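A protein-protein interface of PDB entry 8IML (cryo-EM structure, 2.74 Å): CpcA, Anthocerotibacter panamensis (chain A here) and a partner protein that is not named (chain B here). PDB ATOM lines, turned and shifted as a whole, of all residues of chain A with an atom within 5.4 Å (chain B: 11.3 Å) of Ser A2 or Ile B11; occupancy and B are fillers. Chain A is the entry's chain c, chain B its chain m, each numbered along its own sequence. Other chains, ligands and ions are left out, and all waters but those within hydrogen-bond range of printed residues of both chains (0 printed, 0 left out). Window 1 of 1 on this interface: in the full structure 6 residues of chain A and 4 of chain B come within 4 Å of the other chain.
The backbone carbonyl oxygen (O) of Ser A2 lies close to the backbone carbonyl oxygen (O) of Ile B11 (3.3 Å). The backbone NH of Ser A2 is in hydrogen-bond range of the side-chain hydroxyl of Thr B13, at 2.9 Å. The side-chain hydroxyl (OG1) of Thr B12 is in hydrogen-bond range of the side-chain carboxylate (OD2) of Asp A108, 3.2 Å away.
The backbone carbonyl oxygen (O) of Thr B13 lies within hydrogen-bond range of the guanidinium group (NH2) of Arg B17 (3.3 Å). The side-chain carboxylate (OD2) of Asp A108 is in hydrogen-bond range of the side-chain hydroxyl (OG) of Ser A2, at 2.4 Å. OG1 of Thr B12 is in hydrogen-bond range of OE1 of Gln B14, at 2.8 Å. The side-chain hydroxyl of Thr A4 is in hydrogen-bond range of the side-chain hydroxyl of Thr A7 (2.7 Å).
Ile B11 touches Arg A3 (CG2 to CD, 3.7 Å). CG1 of Ile B11 touches CG2 of Thr A7 (3.6 Å). Glu A8 touches Ile B11. Ala A11 touches Ile B11 (CB to CD1, 3.7 Å). CB of Asp A108 touches OE1 of Gln B14 (3.8 Å).
Of chain B, only Ile B11 and Thr B13 come within 4 Å of Ser A2. Of chain A, only Ser A2, Arg A3, Thr A7, Glu A8 and Ala A11 come within 4 Å of Ile B11. Of chain B, only Ile B11 comes within 4 Å of Arg A3. No residue of chain B comes within 4 Å of Thr A4. Glu A8 touches just one residue of chain B: Ile B11 (3.6 Å). Of the printed residues of chain B, Ala A11 touches Ile B11. No residue of chain B comes within 4 Å of Pro A105. Of the printed residues of chain A, Gln B14 touches Asp A108 (3.8 Å). Of the printed residues of chain B, Asp A108 touches Thr B12 (3.2 Å) and Gln B14 (3.8 Å). Printed residues of chain A within 4 Å of Thr B13: Ser A2 (2.9 Å). Of the printed residues of chain A, Thr B12 touches Asp A108 (3.2 Å). Asp B54 touches none of the printed residues of chain A. Pro B52 touches none of the printed residues of chain A. The nearest residue of chain B that does not touch Ser A2 is Thr B12 (4.03 Å). The nearest printed residue of chain A that does not touch Gln B14 is Ser A2 (6.5 Å).
Of the 14 printed residues of chain B, 4 touch a printed residue of chain A. Printed residues of chain B that touch a printed residue of chain A: Ile B11, Thr B12, Thr B13 and Gln B14. Hydrophobic or aromatic side chains of chain B within 4 Å of the printed part of chain A: Ile B11. Among the printed residues, 8 pairs touch across the chains.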
ATOM      1  N   SER A   2       1.078 -14.164  -0.082  1.00  0.00           N
ATOM      2  CA  SER A   2       2.343 -14.276   0.633  1.00  0.00           C
ATOM      3  C   SER A   2       2.393 -15.571   1.435  1.00  0.00           C
ATOM      4  O   SER A   2       1.842 -16.587   1.020  1.00  0.00           O
ATOM      5  CB  SER A   2       2.549 -13.071   1.550  1.00  0.00           C
ATOM      6  OG  SER A   2       3.845 -13.081   2.122  1.00  0.00           O
ATOM      7  N   ARG A   3       3.058 -15.533   2.587  1.00  0.00           N
ATOM      8  CA  ARG A   3       3.228 -16.717   3.416  1.00  0.00           C
ATOM      9  C   ARG A   3       2.961 -16.384   4.875  1.00  0.00           C
ATOM     10  O   ARG A   3       3.454 -15.375   5.389  1.00  0.00           O
ATOM     11  CB  ARG A   3       4.632 -17.304   3.257  1.00  0.00           C
ATOM     12  CG  ARG A   3       4.839 -18.604   4.013  1.00  0.00           C
ATOM     13  CD  ARG A   3       6.238 -19.152   3.807  1.00  0.00           C
ATOM     14  NE  ARG A   3       7.270 -18.312   4.403  1.00  0.00           N
ATOM     15  CZ  ARG A   3       8.573 -18.489   4.209  1.00  0.00           C
ATOM     16  NH1 ARG A   3       9.001 -19.473   3.430  1.00  0.00           N
ATOM     17  NH2 ARG A   3       9.451 -17.684   4.791  1.00  0.00           N
ATOM     18  N   THR A   4       2.173 -17.233   5.529  1.00  0.00           N
ATOM     19  CA  THR A   4       1.941 -17.196   6.965  1.00  0.00           C
ATOM     20  C   THR A   4       2.024 -18.631   7.467  1.00  0.00           C
ATOM     21  O   THR A   4       2.433 -19.538   6.736  1.00  0.00           O
ATOM     22  CB  THR A   4       0.589 -16.552   7.305  1.00  0.00           C
ATOM     23  OG1 THR A   4      -0.468 -17.319   6.717  1.00  0.00           O
ATOM     24  CG2 THR A   4       0.516 -15.127   6.785  1.00  0.00           C
ATOM     25  N   THR A   7      -0.953 -20.307   5.920  1.00  0.00           N
ATOM     26  CA  THR A   7      -0.611 -20.428   4.508  1.00  0.00           C
ATOM     27  C   THR A   7       0.272 -21.644   4.260  1.00  0.00           C
ATOM     28  O   THR A   7       0.052 -22.394   3.305  1.00  0.00           O
ATOM     29  CB  THR A   7       0.073 -19.147   4.038  1.00  0.00           C
ATOM     30  OG1 THR A   7      -0.848 -18.053   4.126  1.00  0.00           O
ATOM     31  CG2 THR A   7       0.564 -19.280   2.616  1.00  0.00           C
ATOM     32  N   GLU A   8       1.261 -21.872   5.128  1.00  0.00           N
ATOM     33  CA  GLU A   8       2.093 -23.066   5.001  1.00  0.00           C
ATOM     34  C   GLU A   8       1.285 -24.331   5.260  1.00  0.00           C
ATOM     35  O   GLU A   8       1.512 -25.364   4.618  1.00  0.00           O
ATOM     36  CB  GLU A   8       3.283 -22.990   5.955  1.00  0.00           C
ATOM     37  CG  GLU A   8       4.408 -22.095   5.467  1.00  0.00           C
ATOM     38  CD  GLU A   8       5.778 -22.617   5.849  1.00  0.00           C
ATOM     39  OE1 GLU A   8       5.998 -22.904   7.044  1.00  0.00           O
ATOM     40  OE2 GLU A   8       6.635 -22.740   4.951  1.00  0.00           O
ATOM     41  N   ALA A  11      -0.619 -24.973   2.183  1.00  0.00           N
ATOM     42  CA  ALA A  11       0.308 -25.396   1.138  1.00  0.00           C
ATOM     43  C   ALA A  11       0.678 -26.864   1.283  1.00  0.00           C
ATOM     44  O   ALA A  11       0.653 -27.618   0.304  1.00  0.00           O
ATOM     45  CB  ALA A  11       1.562 -24.525   1.165  1.00  0.00           C
ATOM     46  N   GLY A 104       6.842 -14.332   6.095  1.00  0.00           N
ATOM     47  CA  GLY A 104       6.550 -14.292   4.683  1.00  0.00           C
ATOM     48  C   GLY A 104       6.628 -12.915   4.053  1.00  0.00           C
ATOM     49  O   GLY A 104       7.326 -12.718   3.053  1.00  0.00           O
ATOM     50  N   PRO A 105       5.884 -11.942   4.594  1.00  0.00           N
ATOM     51  CA  PRO A 105       5.943 -10.588   4.012  1.00  0.00           C
ATOM     52  C   PRO A 105       7.336  -9.993   4.021  1.00  0.00           C
ATOM     53  O   PRO A 105       7.725  -9.316   3.062  1.00  0.00           O
ATOM     54  CB  PRO A 105       4.975  -9.792   4.894  1.00  0.00           C
ATOM     55  CG  PRO A 105       4.021 -10.807   5.397  1.00  0.00           C
ATOM     56  CD  PRO A 105       4.834 -12.045   5.620  1.00  0.00           C
ATOM     57  N   ASP A 108       9.267 -11.805   1.071  1.00  0.00           N
ATOM     58  CA  ASP A 108       8.960 -11.442  -0.305  1.00  0.00           C
ATOM     59  C   ASP A 108       9.019  -9.945  -0.570  1.00  0.00           C
ATOM     60  O   ASP A 108       9.041  -9.542  -1.738  1.00  0.00           O
ATOM     61  CB  ASP A 108       7.577 -11.970  -0.698  1.00  0.00           C
ATOM     62  CG  ASP A 108       6.527 -11.683   0.344  1.00  0.00           C
ATOM     63  OD1 ASP A 108       6.462 -10.534   0.821  1.00  0.00           O
ATOM     64  OD2 ASP A 108       5.760 -12.607   0.686  1.00  0.00           O
ATOM     65  N   ALA B  10       7.325 -21.445  -3.896  1.00  0.00           N
ATOM     66  CA  ALA B  10       6.143 -21.223  -4.717  1.00  0.00           C
ATOM     67  C   ALA B  10       4.948 -20.832  -3.856  1.00  0.00           C
ATOM     68  O   ALA B  10       3.873 -20.523  -4.369  1.00  0.00           O
ATOM     69  CB  ALA B  10       5.826 -22.462  -5.533  1.00  0.00           C
ATOM     70  N   ILE B  11       5.146 -20.857  -2.536  1.00  0.00           N
ATOM     71  CA  ILE B  11       4.081 -20.489  -1.609  1.00  0.00           C
ATOM     72  C   ILE B  11       3.780 -18.998  -1.676  1.00  0.00           C
ATOM     73  O   ILE B  11       2.623 -18.584  -1.537  1.00  0.00           O
ATOM     74  CB  ILE B  11       4.446 -20.930  -0.180  1.00  0.00           C
ATOM     75  CG1 ILE B  11       3.250 -20.756   0.750  1.00  0.00           C
ATOM     76  CG2 ILE B  11       5.664 -20.175   0.341  1.00  0.00           C
ATOM     77  CD1 ILE B  11       3.417 -21.448   2.067  1.00  0.00           C
ATOM     78  N   THR B  12       4.801 -18.172  -1.887  1.00  0.00           N
ATOM     79  CA  THR B  12       4.648 -16.727  -1.863  1.00  0.00           C
ATOM     80  C   THR B  12       3.764 -16.255  -3.017  1.00  0.00           C
ATOM     81  O   THR B  12       3.345 -17.031  -3.882  1.00  0.00           O
ATOM     82  CB  THR B  12       6.022 -16.062  -1.914  1.00  0.00           C
ATOM     83  OG1 THR B  12       5.882 -14.648  -1.727  1.00  0.00           O
ATOM     84  CG2 THR B  12       6.704 -16.356  -3.241  1.00  0.00           C
ATOM     85  N   THR B  13       3.468 -14.952  -3.016  1.00  0.00           N
ATOM     86  CA  THR B  13       2.634 -14.369  -4.062  1.00  0.00           C
ATOM     87  C   THR B  13       3.244 -14.576  -5.442  1.00  0.00           C
ATOM     88  O   THR B  13       2.515 -14.751  -6.425  1.00  0.00           O
ATOM     89  CB  THR B  13       2.425 -12.877  -3.789  1.00  0.00           C
ATOM     90  OG1 THR B  13       1.694 -12.710  -2.568  1.00  0.00           O
ATOM     91  CG2 THR B  13       1.655 -12.214  -4.922  1.00  0.00           C
ATOM     92  N   GLN B  14       4.572 -14.587  -5.528  1.00  0.00           N
ATOM     93  CA  GLN B  14       5.243 -14.735  -6.810  1.00  0.00           C
ATOM     94  C   GLN B  14       5.138 -16.155  -7.349  1.00  0.00           C
ATOM     95  O   GLN B  14       4.997 -16.339  -8.561  1.00  0.00           O
ATOM     96  CB  GLN B  14       6.701 -14.307  -6.671  1.00  0.00           C
ATOM     97  CG  GLN B  14       6.842 -12.826  -6.385  1.00  0.00           C
ATOM     98  CD  GLN B  14       6.640 -12.501  -4.917  1.00  0.00           C
ATOM     99  OE1 GLN B  14       6.712 -13.382  -4.064  1.00  0.00           O
ATOM    100  NE2 GLN B  14       6.359 -11.239  -4.617  1.00  0.00           N
ATOM    101  N   GLY B  15       5.189 -17.166  -6.479  1.00  0.00           N
ATOM    102  CA  GLY B  15       4.960 -18.532  -6.922  1.00  0.00           C
ATOM    103  C   GLY B  15       3.573 -18.755  -7.488  1.00  0.00           C
ATOM    104  O   GLY B  15       3.340 -19.757  -8.174  1.00  0.00           O
ATOM    105  N   LYS B  16       2.653 -17.837  -7.215  1.00  0.00           N
ATOM    106  CA  LYS B  16       1.312 -17.830  -7.779  1.00  0.00           C
ATOM    107  C   LYS B  16       1.387 -17.251  -9.195  1.00  0.00           C
ATOM    108  O   LYS B  16       2.455 -17.199  -9.809  1.00  0.00           O
ATOM    109  CB  LYS B  16       0.382 -17.050  -6.850  1.00  0.00           C
ATOM    110  CG  LYS B  16      -1.109 -17.172  -7.111  1.00  0.00           C
ATOM    111  CD  LYS B  16      -1.879 -16.452  -6.034  1.00  0.00           C
ATOM    112  CE  LYS B  16      -1.552 -14.971  -6.020  1.00  0.00           C
ATOM    113  NZ  LYS B  16      -2.239 -14.265  -4.902  1.00  0.00           N
ATOM    114  N   ARG B  17       0.239 -16.856  -9.743  1.00  0.00           N
ATOM    115  CA  ARG B  17       0.104 -16.168 -11.031  1.00  0.00           C
ATOM    116  C   ARG B  17       0.821 -16.930 -12.151  1.00  0.00           C
ATOM    117  O   ARG B  17       1.806 -16.488 -12.738  1.00  0.00           O
ATOM    118  CB  ARG B  17       0.530 -14.694 -10.934  1.00  0.00           C
ATOM    119  CG  ARG B  17       1.968 -14.365 -10.565  1.00  0.00           C
ATOM    120  CD  ARG B  17       2.190 -12.864 -10.585  1.00  0.00           C
ATOM    121  NE  ARG B  17       3.603 -12.515 -10.497  1.00  0.00           N
ATOM    122  CZ  ARG B  17       4.225 -12.221  -9.362  1.00  0.00           C
ATOM    123  NH1 ARG B  17       5.514 -11.914  -9.369  1.00  0.00           N
ATOM    124  NH2 ARG B  17       3.556 -12.232  -8.217  1.00  0.00           N
ATOM    125  N   ILE B  18       0.271 -18.118 -12.416  1.00  0.00           N
ATOM    126  CA  ILE B  18       0.698 -18.912 -13.561  1.00  0.00           C
ATOM    127  C   ILE B  18       0.407 -18.159 -14.856  1.00  0.00           C
ATOM    128  O   ILE B  18      -0.443 -17.262 -14.917  1.00  0.00           O
ATOM    129  CB  ILE B  18       0.003 -20.282 -13.549  1.00  0.00           C
ATOM    130  CG1 ILE B  18      -1.493 -20.115 -13.813  1.00  0.00           C
ATOM    131  CG2 ILE B  18       0.219 -20.975 -12.219  1.00  0.00           C
ATOM    132  CD1 ILE B  18      -2.226 -21.414 -14.064  1.00  0.00           C
ATOM    133  N   PRO B  52       4.526 -21.685 -14.237  1.00  0.00           N
ATOM    134  CA  PRO B  52       4.472 -20.779 -13.087  1.00  0.00           C
ATOM    135  C   PRO B  52       5.464 -19.639 -13.250  1.00  0.00           C
ATOM    136  O   PRO B  52       6.346 -19.654 -14.110  1.00  0.00           O
ATOM    137  CB  PRO B  52       4.840 -21.675 -11.899  1.00  0.00           C
ATOM    138  CG  PRO B  52       4.683 -23.077 -12.401  1.00  0.00           C
ATOM    139  CD  PRO B  52       5.006 -23.022 -13.855  1.00  0.00           C
ATOM    140  N   TYR B  53       5.300 -18.630 -12.397  1.00  0.00           N
ATOM    141  CA  TYR B  53       6.140 -17.443 -12.483  1.00  0.00           C
ATOM    142  C   TYR B  53       7.603 -17.774 -12.224  1.00  0.00           C
ATOM    143  O   TYR B  53       8.496 -17.212 -12.870  1.00  0.00           O
ATOM    144  CB  TYR B  53       5.639 -16.389 -11.499  1.00  0.00           C
ATOM    145  CG  TYR B  53       6.462 -15.125 -11.449  1.00  0.00           C
ATOM    146  CD1 TYR B  53       7.554 -15.016 -10.600  1.00  0.00           C
ATOM    147  CD2 TYR B  53       6.131 -14.030 -12.231  1.00  0.00           C
ATOM    148  CE1 TYR B  53       8.303 -13.865 -10.549  1.00  0.00           C
ATOM    149  CE2 TYR B  53       6.873 -12.875 -12.185  1.00  0.00           C
ATOM    150  CZ  TYR B  53       7.956 -12.797 -11.340  1.00  0.00           C
ATOM    151  OH  TYR B  53       8.700 -11.639 -11.292  1.00  0.00           O
ATOM    152  N   ASP B  54       7.872 -18.672 -11.276  1.00  0.00           N
ATOM    153  CA  ASP B  54       9.255 -19.004 -10.947  1.00  0.00           C
ATOM    154  C   ASP B  54       9.972 -19.622 -12.140  1.00  0.00           C
ATOM    155  O   ASP B  54      11.142 -19.317 -12.397  1.00  0.00           O
ATOM    156  CB  ASP B  54       9.298 -19.949  -9.748  1.00  0.00           C
ATOM    157  CG  ASP B  54       9.530 -19.221  -8.440  1.00  0.00           C
ATOM    158  OD1 ASP B  54       9.920 -18.035  -8.478  1.00  0.00           O
ATOM    159  OD2 ASP B  54       9.322 -19.835  -7.373  1.00  0.00           O
ATOM    160  N   ARG B  55       9.290 -20.492 -12.877  1.00  0.00           N
ATOM    161  CA  ARG B  55       9.848 -21.125 -14.062  1.00  0.00           C
ATOM    162  C   ARG B  55       9.536 -20.351 -15.335  1.00  0.00           C
ATOM    163  O   ARG B  55       9.878 -20.813 -16.427  1.00  0.00           O
ATOM    164  CB  ARG B  55       9.327 -22.557 -14.181  1.00  0.00           C
ATOM    165  CG  ARG B  55       9.802 -23.478 -13.075  1.00  0.00           C
ATOM    166  CD  ARG B  55       9.946 -24.903 -13.571  1.00  0.00           C
ATOM    167  NE  ARG B  55      10.498 -24.956 -14.921  1.00  0.00           N
ATOM    168  CZ  ARG B  55      11.792 -24.851 -15.205  1.00  0.00           C
ATOM    169  NH1 ARG B  55      12.200 -24.910 -16.465  1.00  0.00           N
ATOM    170  NH2 ARG B  55      12.677 -24.688 -14.233  1.00  0.00           N
ATOM    171  N   ILE B  77      -3.838 -16.386 -13.945  1.00  0.00           N
ATOM    172  CA  ILE B  77      -4.156 -15.833 -12.636  1.00  0.00           C
ATOM    173  C   ILE B  77      -3.910 -14.333 -12.693  1.00  0.00           C
ATOM    174  O   ILE B  77      -2.825 -13.892 -13.091  1.00  0.00           O
ATOM    175  CB  ILE B  77      -3.319 -16.482 -11.525  1.00  0.00           C
ATOM    176  CG1 ILE B  77      -3.565 -17.986 -11.462  1.00  0.00           C
ATOM    177  CG2 ILE B  77      -3.632 -15.840 -10.182  1.00  0.00           C
ATOM    178  CD1 ILE B  77      -2.754 -18.690 -10.406  1.00  0.00           C
